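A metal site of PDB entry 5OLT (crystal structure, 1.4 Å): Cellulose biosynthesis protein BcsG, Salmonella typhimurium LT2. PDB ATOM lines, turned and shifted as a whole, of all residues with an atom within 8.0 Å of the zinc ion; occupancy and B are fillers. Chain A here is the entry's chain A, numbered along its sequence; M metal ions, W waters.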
ATOM      1  N   ASN A  65      -1.577  12.251  -5.455  1.00  0.00           N
ATOM      2  CA  ASN A  65      -1.926  11.416  -4.318  1.00  0.00           C
ATOM      3  C   ASN A  65      -1.902  12.285  -3.069  1.00  0.00           C
ATOM      4  O   ASN A  65      -0.867  12.799  -2.675  1.00  0.00           O
ATOM      5  CB  ASN A  65      -0.896  10.265  -4.271  1.00  0.00           C
ATOM      6  CG  ASN A  65      -1.162   9.262  -3.188  1.00  0.00           C
ATOM      7  OD1 ASN A  65      -2.305   8.790  -2.996  1.00  0.00           O
ATOM      8  ND2 ASN A  65      -0.108   8.883  -2.501  1.00  0.00           N
ATOM      9  N   ILE A  66      -3.090  12.508  -2.503  1.00  0.00           N
ATOM     10  CA  ILE A  66      -3.272  13.552  -1.481  1.00  0.00           C
ATOM     11  C   ILE A  66      -3.486  12.933  -0.115  1.00  0.00           C
ATOM     12  O   ILE A  66      -4.432  12.167   0.089  1.00  0.00           O
ATOM     13  CB  ILE A  66      -4.488  14.447  -1.822  1.00  0.00           C
ATOM     14  CG1 ILE A  66      -4.309  15.105  -3.203  1.00  0.00           C
ATOM     15  CG2 ILE A  66      -4.748  15.486  -0.709  1.00  0.00           C
ATOM     16  CD1 ILE A  66      -5.549  15.792  -3.727  1.00  0.00           C
ATOM     17  N   CYS A  67      -2.622  13.289   0.833  1.00  0.00           N
ATOM     18  CA  CYS A  67      -2.779  12.826   2.212  1.00  0.00           C
ATOM     19  C   CYS A  67      -4.012  13.475   2.860  1.00  0.00           C
ATOM     20  O   CYS A  67      -4.254  14.668   2.662  1.00  0.00           O
ATOM     21  CB  CYS A  67      -1.491  13.174   3.000  1.00  0.00           C
ATOM     22  SG  CYS A  67      -1.467  12.638   4.744  1.00  0.00           S
ATOM     23  N   SER A  68      -4.759  12.698   3.664  1.00  0.00           N
ATOM     24  CA  SER A  68      -5.715  13.281   4.610  1.00  0.00           C
ATOM     25  C   SER A  68      -6.893  14.013   3.941  1.00  0.00           C
ATOM     26  O   SER A  68      -7.217  15.149   4.318  1.00  0.00           O
ATOM     27  CB  SER A  68      -5.012  14.183   5.645  1.00  0.00           C
ATOM     28  OG  SER A  68      -4.060  13.415   6.383  1.00  0.00           O
ATOM     29  N   LEU A  69      -7.551  13.328   2.998  1.00  0.00           N
ATOM     30  CA  LEU A  69      -8.699  13.872   2.265  1.00  0.00           C
ATOM     31  C   LEU A  69      -9.670  12.734   1.988  1.00  0.00           C
ATOM     32  O   LEU A  69      -9.413  11.908   1.102  1.00  0.00           O
ATOM     33  CB  LEU A  69      -8.202  14.528   0.958  1.00  0.00           C
ATOM     34  CG  LEU A  69      -9.355  15.064   0.074  1.00  0.00           C
ATOM     35  CD1 LEU A  69     -10.117  16.148   0.803  1.00  0.00           C
ATOM     36  CD2 LEU A  69      -8.726  15.623  -1.220  1.00  0.00           C
ATOM     37  N   SER A 100      -5.772   3.458   6.379  1.00  0.00           N
ATOM     38  CA  SER A 100      -5.817   4.813   6.883  1.00  0.00           C
ATOM     39  C   SER A 100      -4.450   5.409   7.174  1.00  0.00           C
ATOM     40  O   SER A 100      -4.391   6.497   7.783  1.00  0.00           O
ATOM     41  CB  SER A 100      -6.732   4.933   8.078  1.00  0.00           C
ATOM     42  OG  SER A 100      -6.362   4.051   9.125  1.00  0.00           O
ATOM     43  N   TYR A 101      -3.369   4.757   6.703  1.00  0.00           N
ATOM     44  CA  TYR A 101      -2.001   5.284   6.884  1.00  0.00           C
ATOM     45  C   TYR A 101      -1.365   5.592   5.555  1.00  0.00           C
ATOM     46  O   TYR A 101      -1.665   4.959   4.543  1.00  0.00           O
ATOM     47  CB  TYR A 101      -1.150   4.267   7.645  1.00  0.00           C
ATOM     48  CG  TYR A 101      -1.545   4.014   9.104  1.00  0.00           C
ATOM     49  CD1 TYR A 101      -2.046   5.041   9.919  1.00  0.00           C
ATOM     50  CD2 TYR A 101      -1.329   2.768   9.668  1.00  0.00           C
ATOM     51  CE1 TYR A 101      -2.366   4.805  11.267  1.00  0.00           C
ATOM     52  CE2 TYR A 101      -1.606   2.522  11.004  1.00  0.00           C
ATOM     53  CZ  TYR A 101      -2.135   3.536  11.794  1.00  0.00           C
ATOM     54  OH  TYR A 101      -2.404   3.227  13.138  1.00  0.00           O
ATOM     55  N   SER A 102      -0.447   6.575   5.557  1.00  0.00           N
ATOM     56  CA  SER A 102       0.102   7.092   4.312  1.00  0.00           C
ATOM     57  C   SER A 102       0.979   6.104   3.560  1.00  0.00           C
ATOM     58  O   SER A 102       0.823   5.941   2.342  1.00  0.00           O
ATOM     59  CB  SER A 102       0.960   8.329   4.602  1.00  0.00           C
ATOM     60  OG  SER A 102       0.214   9.324   5.296  1.00  0.00           O
ATOM     61  N   GLY A 103       1.893   5.425   4.278  1.00  0.00           N
ATOM     62  CA  GLY A 103       2.817   4.501   3.600  1.00  0.00           C
ATOM     63  C   GLY A 103       2.085   3.388   2.889  1.00  0.00           C
ATOM     64  O   GLY A 103       2.262   3.189   1.680  1.00  0.00           O
ATOM     65  N   ALA A 105      -0.988   3.327   1.962  1.00  0.00           N
ATOM     66  CA  ALA A 105      -1.801   3.873   0.878  1.00  0.00           C
ATOM     67  C   ALA A 105      -1.015   4.061  -0.382  1.00  0.00           C
ATOM     68  O   ALA A 105      -1.500   3.728  -1.487  1.00  0.00           O
ATOM     69  CB  ALA A 105      -2.421   5.192   1.286  1.00  0.00           C
ATOM     70  N   ALA A 106       0.177   4.628  -0.247  1.00  0.00           N
ATOM     71  CA  ALA A 106       1.015   4.877  -1.421  1.00  0.00           C
ATOM     72  C   ALA A 106       1.455   3.568  -2.065  1.00  0.00           C
ATOM     73  O   ALA A 106       1.428   3.424  -3.296  1.00  0.00           O
ATOM     74  CB  ALA A 106       2.225   5.697  -1.037  1.00  0.00           C
ATOM     75  N   PHE A 156       8.514   7.702   4.758  1.00  0.00           N
ATOM     76  CA  PHE A 156       7.577   7.603   3.627  1.00  0.00           C
ATOM     77  C   PHE A 156       8.283   7.428   2.283  1.00  0.00           C
ATOM     78  O   PHE A 156       7.935   6.542   1.510  1.00  0.00           O
ATOM     79  CB  PHE A 156       6.678   8.837   3.579  1.00  0.00           C
ATOM     80  CG  PHE A 156       5.684   8.816   2.440  1.00  0.00           C
ATOM     81  CD1 PHE A 156       4.536   8.008   2.511  1.00  0.00           C
ATOM     82  CD2 PHE A 156       5.898   9.591   1.313  1.00  0.00           C
ATOM     83  CE1 PHE A 156       3.625   7.973   1.446  1.00  0.00           C
ATOM     84  CE2 PHE A 156       4.973   9.568   0.257  1.00  0.00           C
ATOM     85  CZ  PHE A 156       3.855   8.762   0.325  1.00  0.00           C
ATOM     86  N   PHE A 183       4.008  19.321  10.455  1.00  0.00           N
ATOM     87  CA  PHE A 183       3.951  18.790  11.804  1.00  0.00           C
ATOM     88  C   PHE A 183       5.333  18.308  12.315  1.00  0.00           C
ATOM     89  O   PHE A 183       5.534  18.243  13.523  1.00  0.00           O
ATOM     90  CB  PHE A 183       2.924  17.650  11.849  1.00  0.00           C
ATOM     91  CG  PHE A 183       3.172  16.594  10.806  1.00  0.00           C
ATOM     92  CD1 PHE A 183       2.762  16.773   9.472  1.00  0.00           C
ATOM     93  CD2 PHE A 183       3.848  15.411  11.147  1.00  0.00           C
ATOM     94  CE1 PHE A 183       3.032  15.804   8.503  1.00  0.00           C
ATOM     95  CE2 PHE A 183       4.093  14.436  10.195  1.00  0.00           C
ATOM     96  CZ  PHE A 183       3.686  14.631   8.864  1.00  0.00           C
ATOM     97  N   ASN A 215       3.075  13.149  -4.528  1.00  0.00           N
ATOM     98  CA  ASN A 215       2.459  13.011  -3.215  1.00  0.00           C
ATOM     99  C   ASN A 215       2.420  14.355  -2.487  1.00  0.00           C
ATOM    100  O   ASN A 215       3.407  15.090  -2.479  1.00  0.00           O
ATOM    101  CB  ASN A 215       3.181  11.948  -2.363  1.00  0.00           C
ATOM    102  CG  ASN A 215       2.507  11.739  -1.043  1.00  0.00           C
ATOM    103  OD1 ASN A 215       2.905  12.315  -0.033  1.00  0.00           O
ATOM    104  ND2 ASN A 215       1.460  10.888  -1.033  1.00  0.00           N
ATOM    105  N   LEU A 216       1.247  14.677  -1.943  1.00  0.00           N
ATOM    106  CA  LEU A 216       0.938  15.992  -1.355  1.00  0.00           C
ATOM    107  C   LEU A 216       0.528  15.884   0.092  1.00  0.00           C
ATOM    108  O   LEU A 216      -0.421  15.179   0.411  1.00  0.00           O
ATOM    109  CB  LEU A 216      -0.247  16.682  -2.091  1.00  0.00           C
ATOM    110  CG  LEU A 216      -0.037  17.039  -3.540  1.00  0.00           C
ATOM    111  CD1 LEU A 216      -0.141  15.807  -4.406  1.00  0.00           C
ATOM    112  CD2 LEU A 216      -1.080  18.072  -3.960  1.00  0.00           C
ATOM    113  N   LEU A 217       1.187  16.669   0.948  1.00  0.00           N
ATOM    114  CA  LEU A 217       0.984  16.651   2.383  1.00  0.00           C
ATOM    115  C   LEU A 217       0.240  17.860   3.043  1.00  0.00           C
ATOM    116  O   LEU A 217       0.135  17.875   4.268  1.00  0.00           O
ATOM    117  CB  LEU A 217       2.417  16.589   3.016  1.00  0.00           C
ATOM    118  CG  LEU A 217       2.562  15.946   4.369  1.00  0.00           C
ATOM    119  CD1 LEU A 217       2.183  14.464   4.291  1.00  0.00           C
ATOM    120  CD2 LEU A 217       3.987  16.113   4.888  1.00  0.00           C
ATOM    121  N   LEU A 219      -2.710  18.787   3.752  1.00  0.00           N
ATOM    122  CA  LEU A 219      -3.885  18.564   4.591  1.00  0.00           C
ATOM    123  C   LEU A 219      -3.557  17.732   5.820  1.00  0.00           C
ATOM    124  O   LEU A 219      -4.428  17.495   6.639  1.00  0.00           O
ATOM    125  CB  LEU A 219      -5.008  17.921   3.770  1.00  0.00           C
ATOM    126  CG  LEU A 219      -5.365  18.703   2.520  1.00  0.00           C
ATOM    127  CD1 LEU A 219      -6.554  17.999   1.857  1.00  0.00           C
ATOM    128  CD2 LEU A 219      -5.650  20.187   2.764  1.00  0.00           C
ATOM    129  N   HIS A 220      -2.291  17.277   5.966  1.00  0.00           N
ATOM    130  CA  HIS A 220      -1.956  16.495   7.161  1.00  0.00           C
ATOM    131  C   HIS A 220      -2.111  17.314   8.433  1.00  0.00           C
ATOM    132  O   HIS A 220      -1.832  18.498   8.464  1.00  0.00           O
ATOM    133  CB  HIS A 220      -0.521  16.001   7.054  1.00  0.00           C
ATOM    134  CG  HIS A 220      -0.161  14.929   8.068  1.00  0.00           C
ATOM    135  ND1 HIS A 220      -0.021  15.184   9.433  1.00  0.00           N
ATOM    136  CD2 HIS A 220       0.097  13.622   7.907  1.00  0.00           C
ATOM    137  CE1 HIS A 220       0.339  14.076  10.048  1.00  0.00           C
ATOM    138  NE2 HIS A 220       0.426  13.107   9.143  1.00  0.00           N
ATOM    139  N   PRO A 265      -6.824  10.353  -3.277  1.00  0.00           N
ATOM    140  CA  PRO A 265      -6.312  10.546  -1.903  1.00  0.00           C
ATOM    141  C   PRO A 265      -5.838   9.235  -1.294  1.00  0.00           C
ATOM    142  O   PRO A 265      -6.282   8.150  -1.657  1.00  0.00           O
ATOM    143  CB  PRO A 265      -7.518  11.070  -1.139  1.00  0.00           C
ATOM    144  CG  PRO A 265      -8.400  11.648  -2.211  1.00  0.00           C
ATOM    145  CD  PRO A 265      -8.246  10.728  -3.395  1.00  0.00           C
ATOM    146  N   GLU A 266      -4.904   9.388  -0.351  1.00  0.00           N
ATOM    147  CA  GLU A 266      -4.383   8.208   0.376  1.00  0.00           C
ATOM    148  C   GLU A 266      -5.393   7.646   1.351  1.00  0.00           C
ATOM    149  O   GLU A 266      -5.461   6.424   1.550  1.00  0.00           O
ATOM    150  CB  GLU A 266      -3.220   8.657   1.269  1.00  0.00           C
ATOM    151  CG  GLU A 266      -1.977   9.239   0.614  1.00  0.00           C
ATOM    152  CD  GLU A 266      -1.062   9.796   1.685  1.00  0.00           C
ATOM    153  OE1 GLU A 266      -1.413   9.641   2.881  1.00  0.00           O
ATOM    154  OE2 GLU A 266      -0.025  10.386   1.358  1.00  0.00           O
ATOM    155  N   HIS A 267      -6.101   8.542   2.055  1.00  0.00           N
ATOM    156  CA  HIS A 267      -6.974   8.212   3.216  1.00  0.00           C
ATOM    157  C   HIS A 267      -7.432   9.552   3.750  1.00  0.00           C
ATOM    158  O   HIS A 267      -6.811  10.599   3.447  1.00  0.00           O
ATOM    159  CB  HIS A 267      -6.158   7.487   4.362  1.00  0.00           C
ATOM    160  CG  HIS A 267      -5.015   8.312   4.884  1.00  0.00           C
ATOM    161  ND1 HIS A 267      -5.199   9.346   5.783  1.00  0.00           N
ATOM    162  CD2 HIS A 267      -3.698   8.320   4.562  1.00  0.00           C
ATOM    163  CE1 HIS A 267      -4.036   9.978   5.967  1.00  0.00           C
ATOM    164  NE2 HIS A 267      -3.108   9.359   5.249  1.00  0.00           N
ATOM    165  N   GLY A 268      -8.468   9.516   4.571  1.00  0.00           N
ATOM    166  CA  GLY A 268      -8.971  10.737   5.172  1.00  0.00           C
ATOM    167  C   GLY A 268      -8.163  11.278   6.327  1.00  0.00           C
ATOM    168  O   GLY A 268      -7.331  10.583   6.922  1.00  0.00           O
ATOM    169  N   GLY A 269      -8.450  12.521   6.685  1.00  0.00           N
ATOM    170  CA  GLY A 269      -7.788  13.170   7.837  1.00  0.00           C
ATOM    171  C   GLY A 269      -8.503  13.015   9.159  1.00  0.00           C
ATOM    172  O   GLY A 269      -8.058  13.531  10.164  1.00  0.00           O
ATOM    173  N   ARG A 282      -6.938   8.009  13.572  1.00  0.00           N
ATOM    174  CA  ARG A 282      -7.293   7.186  12.372  1.00  0.00           C
ATOM    175  C   ARG A 282      -6.568   5.841  12.420  1.00  0.00           C
ATOM    176  O   ARG A 282      -6.174   5.305  11.399  1.00  0.00           O
ATOM    177  CB  ARG A 282      -7.082   7.987  11.072  1.00  0.00           C
ATOM    178  CG  ARG A 282      -5.711   8.609  10.957  1.00  0.00           C
ATOM    179  CD  ARG A 282      -5.588   9.289   9.598  1.00  0.00           C
ATOM    180  NE  ARG A 282      -4.439  10.182   9.593  1.00  0.00           N
ATOM    181  CZ  ARG A 282      -3.190   9.874   9.277  1.00  0.00           C
ATOM    182  NH1 ARG A 282      -2.849   8.648   8.864  1.00  0.00           N
ATOM    183  NH2 ARG A 282      -2.236  10.818   9.404  1.00  0.00           N
HETATM  184 ZN    ZN M   1      -1.374  10.358   4.662  1.00  0.00          ZN
HETATM  185  O   HOH W   1      -0.825  10.626   7.083  1.00  0.00           O
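Within 4 Å of the zinc ion: Cys 67, Ser 102, Glu 266 and His 267.
Along chain A the residues within 4 Å of the zinc ion span positions 67 to 267.
The backbone carbonyl oxygen (O) of His 267 lies within hydrogen-bond range of the backbone NH (N) of Leu 69.
N of Ser 68 lies within hydrogen-bond range of O of His 267, 2.9 Å away.
The side-chain amide nitrogen of Asn 215 lies within hydrogen-bond range of the side-chain carboxylate of Glu 266, 2.9 Å away.
N of Cys 67 sits at hydrogen-bond distance from O of Leu 216.
O of Ile 66 is in hydrogen-bond range of N of Glu 266 (2.9 Å).
The side-chain sulfur (SG) of Cys 67 lies close to the side-chain hydroxyl (OG) of Ser 68 (3.2 Å).
Water W1 lies within hydrogen-bond range of the guanidinium group of Arg 282 and a ring nitrogen (NE2) of His 220.
The zinc ion is bound by the side-chain carboxylate (OE1) of Glu 266 (1.9 Å), the side-chain hydroxyl (OG) of Ser 102 (2.0 Å), a ring nitrogen (NE2) of His 267 (2.1 Å), the side-chain sulfur (SG) of Cys 67 (2.3 Å) and water W1 (2.5 Å).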
